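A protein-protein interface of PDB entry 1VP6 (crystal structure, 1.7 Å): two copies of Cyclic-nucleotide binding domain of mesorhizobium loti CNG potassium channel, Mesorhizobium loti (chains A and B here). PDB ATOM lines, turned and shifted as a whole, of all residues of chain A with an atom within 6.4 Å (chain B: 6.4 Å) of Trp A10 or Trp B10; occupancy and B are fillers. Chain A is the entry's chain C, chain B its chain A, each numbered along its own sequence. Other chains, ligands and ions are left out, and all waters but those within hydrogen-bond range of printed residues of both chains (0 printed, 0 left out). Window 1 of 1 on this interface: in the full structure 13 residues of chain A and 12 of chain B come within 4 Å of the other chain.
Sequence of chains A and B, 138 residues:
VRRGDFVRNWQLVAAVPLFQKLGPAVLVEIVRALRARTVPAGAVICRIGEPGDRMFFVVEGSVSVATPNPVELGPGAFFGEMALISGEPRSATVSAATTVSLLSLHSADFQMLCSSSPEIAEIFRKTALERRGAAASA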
ATOM      1  N   ASP A   5      -3.109  -6.583 -31.681  1.00  0.00           N
ATOM      2  CA  ASP A   5      -4.054  -7.491 -31.036  1.00  0.00           C
ATOM      3  C   ASP A   5      -3.642  -7.772 -29.597  1.00  0.00           C
ATOM      4  O   ASP A   5      -4.478  -7.836 -28.694  1.00  0.00           O
ATOM      5  CB  ASP A   5      -4.130  -8.805 -31.816  1.00  0.00           C
ATOM      6  CG  ASP A   5      -4.756  -8.634 -33.187  1.00  0.00           C
ATOM      7  OD1 ASP A   5      -4.614  -9.548 -34.025  1.00  0.00           O
ATOM      8  OD2 ASP A   5      -5.399  -7.589 -33.422  1.00  0.00           O
ATOM      9  N   PHE A   6      -2.341  -7.940 -29.394  1.00  0.00           N
ATOM     10  CA  PHE A   6      -1.799  -8.220 -28.072  1.00  0.00           C
ATOM     11  C   PHE A   6      -2.117  -7.090 -27.094  1.00  0.00           C
ATOM     12  O   PHE A   6      -2.670  -7.320 -26.015  1.00  0.00           O
ATOM     13  CB  PHE A   6      -0.286  -8.405 -28.171  1.00  0.00           C
ATOM     14  CG  PHE A   6       0.375  -8.723 -26.863  1.00  0.00           C
ATOM     15  CD1 PHE A   6       0.237  -9.981 -26.285  1.00  0.00           C
ATOM     16  CD2 PHE A   6       1.141  -7.764 -26.209  1.00  0.00           C
ATOM     17  CE1 PHE A   6       0.858 -10.279 -25.075  1.00  0.00           C
ATOM     18  CE2 PHE A   6       1.765  -8.051 -25.000  1.00  0.00           C
ATOM     19  CZ  PHE A   6       1.624  -9.311 -24.432  1.00  0.00           C
ATOM     20  N   VAL A   7      -1.753  -5.868 -27.466  1.00  0.00           N
ATOM     21  CA  VAL A   7      -2.004  -4.723 -26.605  1.00  0.00           C
ATOM     22  C   VAL A   7      -3.494  -4.518 -26.351  1.00  0.00           C
ATOM     23  O   VAL A   7      -3.903  -4.264 -25.218  1.00  0.00           O
ATOM     24  CB  VAL A   7      -1.401  -3.435 -27.197  1.00  0.00           C
ATOM     25  CG1 VAL A   7      -1.774  -2.243 -26.332  1.00  0.00           C
ATOM     26  CG2 VAL A   7       0.116  -3.569 -27.275  1.00  0.00           C
ATOM     27  N   ARG A   8      -4.307  -4.633 -27.396  1.00  0.00           N
ATOM     28  CA  ARG A   8      -5.749  -4.460 -27.247  1.00  0.00           C
ATOM     29  C   ARG A   8      -6.352  -5.472 -26.273  1.00  0.00           C
ATOM     30  O   ARG A   8      -7.275  -5.145 -25.522  1.00  0.00           O
ATOM     31  CB  ARG A   8      -6.439  -4.579 -28.610  1.00  0.00           C
ATOM     32  CG  ARG A   8      -7.960  -4.457 -28.572  1.00  0.00           C
ATOM     33  CD  ARG A   8      -8.409  -3.173 -27.883  1.00  0.00           C
ATOM     34  NE  ARG A   8      -9.857  -2.992 -27.952  1.00  0.00           N
ATOM     35  CZ  ARG A   8     -10.522  -2.042 -27.303  1.00  0.00           C
ATOM     36  NH1 ARG A   8      -9.871  -1.183 -26.528  1.00  0.00           N
ATOM     37  NH2 ARG A   8     -11.839  -1.948 -27.429  1.00  0.00           N
ATOM     38  N   ASN A   9      -5.836  -6.697 -26.283  1.00  0.00           N
ATOM     39  CA  ASN A   9      -6.348  -7.735 -25.391  1.00  0.00           C
ATOM     40  C   ASN A   9      -6.248  -7.386 -23.909  1.00  0.00           C
ATOM     41  O   ASN A   9      -7.095  -7.806 -23.114  1.00  0.00           O
ATOM     42  CB  ASN A   9      -5.637  -9.064 -25.639  1.00  0.00           C
ATOM     43  CG  ASN A   9      -6.326  -9.902 -26.692  1.00  0.00           C
ATOM     44  OD1 ASN A   9      -7.336  -9.493 -27.267  1.00  0.00           O
ATOM     45  ND2 ASN A   9      -5.789 -11.091 -26.944  1.00  0.00           N
ATOM     46  N   TRP A  10      -5.225  -6.630 -23.527  1.00  0.00           N
ATOM     47  CA  TRP A  10      -5.082  -6.264 -22.121  1.00  0.00           C
ATOM     48  C   TRP A  10      -6.253  -5.406 -21.661  1.00  0.00           C
ATOM     49  O   TRP A  10      -6.741  -5.561 -20.544  1.00  0.00           O
ATOM     50  CB  TRP A  10      -3.757  -5.536 -21.877  1.00  0.00           C
ATOM     51  CG  TRP A  10      -2.579  -6.439 -21.976  1.00  0.00           C
ATOM     52  CD1 TRP A  10      -1.682  -6.514 -23.001  1.00  0.00           C
ATOM     53  CD2 TRP A  10      -2.198  -7.447 -21.031  1.00  0.00           C
ATOM     54  NE1 TRP A  10      -0.765  -7.511 -22.756  1.00  0.00           N
ATOM     55  CE2 TRP A  10      -1.060  -8.099 -21.554  1.00  0.00           C
ATOM     56  CE3 TRP A  10      -2.711  -7.863 -19.794  1.00  0.00           C
ATOM     57  CZ2 TRP A  10      -0.421  -9.150 -20.883  1.00  0.00           C
ATOM     58  CZ3 TRP A  10      -2.075  -8.913 -19.125  1.00  0.00           C
ATOM     59  CH2 TRP A  10      -0.942  -9.542 -19.674  1.00  0.00           C
ATOM     60  N   GLN A  11      -6.713  -4.511 -22.529  1.00  0.00           N
ATOM     61  CA  GLN A  11      -7.840  -3.648 -22.201  1.00  0.00           C
ATOM     62  C   GLN A  11      -9.107  -4.501 -22.093  1.00  0.00           C
ATOM     63  O   GLN A  11      -9.940  -4.293 -21.208  1.00  0.00           O
ATOM     64  CB  GLN A  11      -8.010  -2.574 -23.286  1.00  0.00           C
ATOM     65  CG  GLN A  11      -6.781  -1.680 -23.463  1.00  0.00           C
ATOM     66  CD  GLN A  11      -6.926  -0.642 -24.569  1.00  0.00           C
ATOM     67  OE1 GLN A  11      -7.234  -0.966 -25.717  1.00  0.00           O
ATOM     68  NE2 GLN A  11      -6.686   0.619 -24.222  1.00  0.00           N
ATOM     69  N   LEU A  12      -9.235  -5.478 -22.984  1.00  0.00           N
ATOM     70  CA  LEU A  12     -10.402  -6.359 -22.994  1.00  0.00           C
ATOM     71  C   LEU A  12     -10.451  -7.335 -21.815  1.00  0.00           C
ATOM     72  O   LEU A  12     -11.510  -7.550 -21.225  1.00  0.00           O
ATOM     73  CB  LEU A  12     -10.449  -7.132 -24.315  1.00  0.00           C
ATOM     74  CG  LEU A  12     -10.455  -6.239 -25.563  1.00  0.00           C
ATOM     75  CD1 LEU A  12     -10.317  -7.097 -26.808  1.00  0.00           C
ATOM     76  CD2 LEU A  12     -11.741  -5.423 -25.605  1.00  0.00           C
ATOM     77  N   VAL A  13      -9.314  -7.930 -21.464  1.00  0.00           N
ATOM     78  CA  VAL A  13      -9.293  -8.872 -20.349  1.00  0.00           C
ATOM     79  C   VAL A  13      -9.662  -8.200 -19.030  1.00  0.00           C
ATOM     80  O   VAL A  13     -10.112  -8.861 -18.097  1.00  0.00           O
ATOM     81  CB  VAL A  13      -7.911  -9.546 -20.195  1.00  0.00           C
ATOM     82  CG1 VAL A  13      -7.634 -10.434 -21.392  1.00  0.00           C
ATOM     83  CG2 VAL A  13      -6.834  -8.493 -20.050  1.00  0.00           C
ATOM     84  N   ALA A  14      -9.488  -6.881 -18.961  1.00  0.00           N
ATOM     85  CA  ALA A  14      -9.811  -6.139 -17.744  1.00  0.00           C
ATOM     86  C   ALA A  14     -11.314  -6.175 -17.463  1.00  0.00           C
ATOM     87  O   ALA A  14     -11.748  -5.944 -16.336  1.00  0.00           O
ATOM     88  CB  ALA A  14      -9.336  -4.693 -17.871  1.00  0.00           C
ATOM     89  N   ALA A  15     -12.104  -6.474 -18.491  1.00  0.00           N
ATOM     90  CA  ALA A  15     -13.555  -6.540 -18.343  1.00  0.00           C
ATOM     91  C   ALA A  15     -14.018  -7.916 -17.861  1.00  0.00           C
ATOM     92  O   ALA A  15     -15.208  -8.126 -17.616  1.00  0.00           O
ATOM     93  CB  ALA A  15     -14.230  -6.199 -19.670  1.00  0.00           C
ATOM     94  N   PRO A  24       0.855 -12.874 -13.261  1.00  0.00           N
ATOM     95  CA  PRO A  24       1.442 -12.280 -14.470  1.00  0.00           C
ATOM     96  C   PRO A  24       1.824 -13.257 -15.585  1.00  0.00           C
ATOM     97  O   PRO A  24       1.431 -13.073 -16.740  1.00  0.00           O
ATOM     98  CB  PRO A  24       2.651 -11.524 -13.926  1.00  0.00           C
ATOM     99  CG  PRO A  24       2.170 -11.077 -12.580  1.00  0.00           C
ATOM    100  CD  PRO A  24       1.489 -12.321 -12.050  1.00  0.00           C
ATOM    101  N   LEU A  27      -1.296 -14.786 -17.078  1.00  0.00           N
ATOM    102  CA  LEU A  27      -2.069 -13.767 -17.782  1.00  0.00           C
ATOM    103  C   LEU A  27      -1.490 -13.563 -19.173  1.00  0.00           C
ATOM    104  O   LEU A  27      -2.227 -13.465 -20.151  1.00  0.00           O
ATOM    105  CB  LEU A  27      -2.038 -12.430 -17.036  1.00  0.00           C
ATOM    106  CG  LEU A  27      -3.027 -12.179 -15.901  1.00  0.00           C
ATOM    107  CD1 LEU A  27      -2.664 -10.877 -15.203  1.00  0.00           C
ATOM    108  CD2 LEU A  27      -4.449 -12.116 -16.456  1.00  0.00           C
ATOM    109  N   VAL A  28      -0.166 -13.489 -19.262  1.00  0.00           N
ATOM    110  CA  VAL A  28       0.479 -13.287 -20.555  1.00  0.00           C
ATOM    111  C   VAL A  28       0.145 -14.421 -21.519  1.00  0.00           C
ATOM    112  O   VAL A  28      -0.187 -14.180 -22.677  1.00  0.00           O
ATOM    113  CB  VAL A  28       2.014 -13.171 -20.408  1.00  0.00           C
ATOM    114  CG1 VAL A  28       2.670 -13.139 -21.780  1.00  0.00           C
ATOM    115  CG2 VAL A  28       2.359 -11.904 -19.642  1.00  0.00           C
ATOM    116  N   GLU A  29       0.228 -15.656 -21.039  1.00  0.00           N
ATOM    117  CA  GLU A  29      -0.087 -16.807 -21.876  1.00  0.00           C
ATOM    118  C   GLU A  29      -1.512 -16.701 -22.411  1.00  0.00           C
ATOM    119  O   GLU A  29      -1.765 -16.955 -23.591  1.00  0.00           O
ATOM    120  CB  GLU A  29       0.064 -18.108 -21.079  1.00  0.00           C
ATOM    121  CG  GLU A  29       1.496 -18.433 -20.676  1.00  0.00           C
ATOM    122  CD  GLU A  29       1.601 -19.714 -19.865  1.00  0.00           C
ATOM    123  OE1 GLU A  29       1.157 -20.775 -20.359  1.00  0.00           O
ATOM    124  OE2 GLU A  29       2.129 -19.663 -18.733  1.00  0.00           O
ATOM    125  N   VAL A  31      -3.424 -13.908 -22.657  1.00  0.00           N
ATOM    126  CA  VAL A  31      -3.570 -12.744 -23.524  1.00  0.00           C
ATOM    127  C   VAL A  31      -3.075 -13.078 -24.928  1.00  0.00           C
ATOM    128  O   VAL A  31      -3.633 -12.612 -25.918  1.00  0.00           O
ATOM    129  CB  VAL A  31      -2.782 -11.531 -22.965  1.00  0.00           C
ATOM    130  CG1 VAL A  31      -2.673 -10.427 -24.018  1.00  0.00           C
ATOM    131  CG2 VAL A  31      -3.489 -10.990 -21.733  1.00  0.00           C
ATOM    132  N   ASP B   5       0.061  -4.484  -9.702  1.00  0.00           N
ATOM    133  CA  ASP B   5       0.964  -3.521 -10.325  1.00  0.00           C
ATOM    134  C   ASP B   5       1.218  -3.898 -11.779  1.00  0.00           C
ATOM    135  O   ASP B   5       1.352  -3.033 -12.644  1.00  0.00           O
ATOM    136  CB  ASP B   5       2.295  -3.459  -9.570  1.00  0.00           C
ATOM    137  CG  ASP B   5       2.138  -2.936  -8.156  1.00  0.00           C
ATOM    138  OD1 ASP B   5       1.351  -1.985  -7.960  1.00  0.00           O
ATOM    139  OD2 ASP B   5       2.808  -3.465  -7.244  1.00  0.00           O
ATOM    140  N   PHE B   6       1.280  -5.200 -12.042  1.00  0.00           N
ATOM    141  CA  PHE B   6       1.513  -5.695 -13.393  1.00  0.00           C
ATOM    142  C   PHE B   6       0.387  -5.270 -14.342  1.00  0.00           C
ATOM    143  O   PHE B   6       0.632  -4.628 -15.361  1.00  0.00           O
ATOM    144  CB  PHE B   6       1.627  -7.224 -13.378  1.00  0.00           C
ATOM    145  CG  PHE B   6       1.861  -7.832 -14.734  1.00  0.00           C
ATOM    146  CD1 PHE B   6       3.086  -7.682 -15.380  1.00  0.00           C
ATOM    147  CD2 PHE B   6       0.854  -8.557 -15.367  1.00  0.00           C
ATOM    148  CE1 PHE B   6       3.306  -8.249 -16.640  1.00  0.00           C
ATOM    149  CE2 PHE B   6       1.064  -9.126 -16.625  1.00  0.00           C
ATOM    150  CZ  PHE B   6       2.289  -8.973 -17.262  1.00  0.00           C
ATOM    151  N   VAL B   7      -0.846  -5.629 -14.007  1.00  0.00           N
ATOM    152  CA  VAL B   7      -1.976  -5.274 -14.858  1.00  0.00           C
ATOM    153  C   VAL B   7      -2.140  -3.760 -14.979  1.00  0.00           C
ATOM    154  O   VAL B   7      -2.515  -3.252 -16.035  1.00  0.00           O
ATOM    155  CB  VAL B   7      -3.291  -5.898 -14.333  1.00  0.00           C
ATOM    156  CG1 VAL B   7      -3.183  -7.422 -14.362  1.00  0.00           C
ATOM    157  CG2 VAL B   7      -3.581  -5.413 -12.921  1.00  0.00           C
ATOM    158  N   ARG B   8      -1.844  -3.043 -13.900  1.00  0.00           N
ATOM    159  CA  ARG B   8      -1.960  -1.587 -13.886  1.00  0.00           C
ATOM    160  C   ARG B   8      -0.974  -0.938 -14.857  1.00  0.00           C
ATOM    161  O   ARG B   8      -1.267   0.095 -15.465  1.00  0.00           O
ATOM    162  CB  ARG B   8      -1.687  -1.064 -12.478  1.00  0.00           C
ATOM    163  CG  ARG B   8      -2.697  -0.063 -11.961  1.00  0.00           C
ATOM    164  CD  ARG B   8      -3.280  -0.564 -10.656  1.00  0.00           C
ATOM    165  NE  ARG B   8      -2.229  -0.928  -9.710  1.00  0.00           N
ATOM    166  CZ  ARG B   8      -2.432  -1.645  -8.610  1.00  0.00           C
ATOM    167  NH1 ARG B   8      -3.651  -2.079  -8.317  1.00  0.00           N
ATOM    168  NH2 ARG B   8      -1.418  -1.932  -7.804  1.00  0.00           N
ATOM    169  N   ASN B   9       0.195  -1.546 -15.003  1.00  0.00           N
ATOM    170  CA  ASN B   9       1.214  -0.999 -15.888  1.00  0.00           C
ATOM    171  C   ASN B   9       0.864  -0.995 -17.375  1.00  0.00           C
ATOM    172  O   ASN B   9       1.388  -0.176 -18.123  1.00  0.00           O
ATOM    173  CB  ASN B   9       2.543  -1.728 -15.686  1.00  0.00           C
ATOM    174  CG  ASN B   9       3.374  -1.127 -14.569  1.00  0.00           C
ATOM    175  OD1 ASN B   9       3.017  -0.096 -13.993  1.00  0.00           O
ATOM    176  ND2 ASN B   9       4.496  -1.762 -14.267  1.00  0.00           N
ATOM    177  N   TRP B  10      -0.012  -1.893 -17.815  1.00  0.00           N
ATOM    178  CA  TRP B  10      -0.351  -1.923 -19.231  1.00  0.00           C
ATOM    179  C   TRP B  10      -0.988  -0.637 -19.737  1.00  0.00           C
ATOM    180  O   TRP B  10      -0.633  -0.145 -20.809  1.00  0.00           O
ATOM    181  CB  TRP B  10      -1.245  -3.127 -19.547  1.00  0.00           C
ATOM    182  CG  TRP B  10      -0.474  -4.409 -19.506  1.00  0.00           C
ATOM    183  CD1 TRP B  10      -0.460  -5.331 -18.500  1.00  0.00           C
ATOM    184  CD2 TRP B  10       0.470  -4.867 -20.484  1.00  0.00           C
ATOM    185  NE1 TRP B  10       0.440  -6.334 -18.788  1.00  0.00           N
ATOM    186  CE2 TRP B  10       1.024  -6.073 -19.999  1.00  0.00           C
ATOM    187  CE3 TRP B  10       0.903  -4.370 -21.722  1.00  0.00           C
ATOM    188  CZ2 TRP B  10       1.990  -6.794 -20.710  1.00  0.00           C
ATOM    189  CZ3 TRP B  10       1.863  -5.087 -22.430  1.00  0.00           C
ATOM    190  CH2 TRP B  10       2.397  -6.287 -21.920  1.00  0.00           C
ATOM    191  N   GLN B  11      -1.912  -0.075 -18.968  1.00  0.00           N
ATOM    192  CA  GLN B  11      -2.561   1.153 -19.397  1.00  0.00           C
ATOM    193  C   GLN B  11      -1.635   2.346 -19.197  1.00  0.00           C
ATOM    194  O   GLN B  11      -1.724   3.333 -19.927  1.00  0.00           O
ATOM    195  CB  GLN B  11      -3.870   1.358 -18.639  1.00  0.00           C
ATOM    196  CG  GLN B  11      -4.864   2.237 -19.383  1.00  0.00           C
ATOM    197  CD  GLN B  11      -5.018   1.827 -20.841  1.00  0.00           C
ATOM    198  OE1 GLN B  11      -5.204   0.650 -21.152  1.00  0.00           O
ATOM    199  NE2 GLN B  11      -4.939   2.801 -21.742  1.00  0.00           N
ATOM    200  N   LEU B  12      -0.745   2.257 -18.213  1.00  0.00           N
ATOM    201  CA  LEU B  12       0.202   3.339 -17.954  1.00  0.00           C
ATOM    202  C   LEU B  12       1.211   3.385 -19.097  1.00  0.00           C
ATOM    203  O   LEU B  12       1.568   4.455 -19.582  1.00  0.00           O
ATOM    204  CB  LEU B  12       0.923   3.115 -16.616  1.00  0.00           C
ATOM    205  CG  LEU B  12       0.044   3.130 -15.359  1.00  0.00           C
ATOM    206  CD1 LEU B  12       0.897   2.821 -14.138  1.00  0.00           C
ATOM    207  CD2 LEU B  12      -0.630   4.490 -15.207  1.00  0.00           C
ATOM    208  N   VAL B  13       1.662   2.212 -19.530  1.00  0.00           N
ATOM    209  CA  VAL B  13       2.619   2.114 -20.626  1.00  0.00           C
ATOM    210  C   VAL B  13       2.013   2.638 -21.929  1.00  0.00           C
ATOM    211  O   VAL B  13       2.724   3.142 -22.799  1.00  0.00           O
ATOM    212  CB  VAL B  13       3.077   0.643 -20.817  1.00  0.00           C
ATOM    213  CG1 VAL B  13       3.686   0.446 -22.193  1.00  0.00           C
ATOM    214  CG2 VAL B  13       4.096   0.280 -19.744  1.00  0.00           C
ATOM    215  N   ALA B  14       0.695   2.521 -22.059  1.00  0.00           N
ATOM    216  CA  ALA B  14       0.015   2.989 -23.261  1.00  0.00           C
ATOM    217  C   ALA B  14       0.151   4.502 -23.441  1.00  0.00           C
ATOM    218  O   ALA B  14       0.047   5.012 -24.558  1.00  0.00           O
ATOM    219  CB  ALA B  14      -1.463   2.598 -23.208  1.00  0.00           C
ATOM    220  N   ALA B  15       0.385   5.214 -22.342  1.00  0.00           N
ATOM    221  CA  ALA B  15       0.527   6.669 -22.379  1.00  0.00           C
ATOM    222  C   ALA B  15       1.903   7.127 -22.864  1.00  0.00           C
ATOM    223  O   ALA B  15       2.132   8.319 -23.050  1.00  0.00           O
ATOM    224  CB  ALA B  15       0.254   7.253 -20.992  1.00  0.00           C
ATOM    225  N   PRO B  24       5.525  -7.669 -28.418  1.00  0.00           N
ATOM    226  CA  PRO B  24       4.954  -8.343 -27.246  1.00  0.00           C
ATOM    227  C   PRO B  24       5.942  -8.813 -26.176  1.00  0.00           C
ATOM    228  O   PRO B  24       5.796  -8.474 -24.999  1.00  0.00           O
ATOM    229  CB  PRO B  24       4.181  -9.508 -27.863  1.00  0.00           C
ATOM    230  CG  PRO B  24       3.719  -8.934 -29.168  1.00  0.00           C
ATOM    231  CD  PRO B  24       4.979  -8.242 -29.661  1.00  0.00           C
ATOM    232  N   LEU B  27       7.577  -5.884 -24.487  1.00  0.00           N
ATOM    233  CA  LEU B  27       6.592  -5.108 -23.740  1.00  0.00           C
ATOM    234  C   LEU B  27       6.371  -5.760 -22.380  1.00  0.00           C
ATOM    235  O   LEU B  27       6.286  -5.079 -21.361  1.00  0.00           O
ATOM    236  CB  LEU B  27       5.259  -5.034 -24.493  1.00  0.00           C
ATOM    237  CG  LEU B  27       5.166  -3.992 -25.609  1.00  0.00           C
ATOM    238  CD1 LEU B  27       3.851  -4.162 -26.366  1.00  0.00           C
ATOM    239  CD2 LEU B  27       5.263  -2.594 -25.001  1.00  0.00           C
ATOM    240  N   VAL B  28       6.283  -7.086 -22.363  1.00  0.00           N
ATOM    241  CA  VAL B  28       6.078  -7.796 -21.106  1.00  0.00           C
ATOM    242  C   VAL B  28       7.258  -7.546 -20.174  1.00  0.00           C
ATOM    243  O   VAL B  28       7.084  -7.368 -18.969  1.00  0.00           O
ATOM    244  CB  VAL B  28       5.911  -9.311 -21.338  1.00  0.00           C
ATOM    245  CG1 VAL B  28       5.852 -10.038 -20.002  1.00  0.00           C
ATOM    246  CG2 VAL B  28       4.632  -9.568 -22.131  1.00  0.00           C
ATOM    247  N   GLU B  29       8.461  -7.525 -20.738  1.00  0.00           N
ATOM    248  CA  GLU B  29       9.659  -7.278 -19.948  1.00  0.00           C
ATOM    249  C   GLU B  29       9.616  -5.911 -19.272  1.00  0.00           C
ATOM    250  O   GLU B  29       9.913  -5.786 -18.082  1.00  0.00           O
ATOM    251  CB  GLU B  29      10.907  -7.369 -20.836  1.00  0.00           C
ATOM    252  CG  GLU B  29      11.269  -8.789 -21.259  1.00  0.00           C
ATOM    253  CD  GLU B  29      12.463  -8.838 -22.198  1.00  0.00           C
ATOM    254  OE1 GLU B  29      13.529  -8.288 -21.845  1.00  0.00           O
ATOM    255  OE2 GLU B  29      12.337  -9.430 -23.291  1.00  0.00           O
ATOM    256  N   VAL B  31       6.900  -3.997 -18.779  1.00  0.00           N
ATOM    257  CA  VAL B  31       5.744  -3.910 -17.890  1.00  0.00           C
ATOM    258  C   VAL B  31       6.062  -4.530 -16.528  1.00  0.00           C
ATOM    259  O   VAL B  31       5.605  -4.049 -15.489  1.00  0.00           O
ATOM    260  CB  VAL B  31       4.516  -4.614 -18.513  1.00  0.00           C
ATOM    261  CG1 VAL B  31       3.393  -4.727 -17.489  1.00  0.00           C
ATOM    262  CG2 VAL B  31       4.036  -3.827 -19.721  1.00  0.00           C
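The side-chain amide oxygen (OE1) of Gln A11 lies within hydrogen-bond range of the guanidinium group (NH1) of Arg A8 (2.8 Å).
Printed residues of chain A within 4 Å of Pro B24: Phe A6. Printed residues of chain A within 4 Å of Leu B27: Val A7. Ala A14 touches none of the printed residues of chain B.
Phe A6 touches Trp B10, and with the chains exchanged Trp A10 touches Phe B6. Phe A6 touches Val B28, and with the chains exchanged Val A28 touches Phe B6. Trp B10 touches its own counterpart, Trp A10. Val B28 touches its own counterpart, Val A28. 16 positions are printed for both chains. Of the 11 pairs that touch across the chains among the printed residues, 11 have their exchanged pair printed and touching as well.
Trp B10 touches Phe A6. CD2 of Phe A6 touches CB of Pro B24, at 3.9 Å. Val B28 touches Phe A6 (CG2 to CZ, 3.8 Å). Val A7 touches Leu B27 (CG2 to CD1, 3.9 Å). Phe B6 touches Trp A10 (CE2 to CH2, 3.7 Å). Trp B10 touches Trp A10 (CE2 to CE2, 3.3 Å). Pro A24 touches Phe B6 (CB to CD2, 3.8 Å). CD1 of Leu A27 touches CG1 of Val B7 (3.6 Å). Val A28 touches Phe B6. CG2 of Val A28 touches CG1 of Val B28 (3.98 Å).
OE1 of Gln B11 is in hydrogen-bond range of NE2 of Gln A11, at 3.4 Å.
Of the 16 printed residues of chain B, 7 touch a printed residue of chain A. Hydrophobic or aromatic side chains of chain A within 4 Å of the printed part of chain B: Phe A6, Val A7, Trp A10, Pro A24, Leu A27 and Val A28. Along chain A the printed residues that touch a printed residue of chain B span positions 6 to 28. Among the printed residues, no Asp or Glu carboxylate lies within 4 Å of a Lys or Arg side-chain nitrogen of the other chain.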
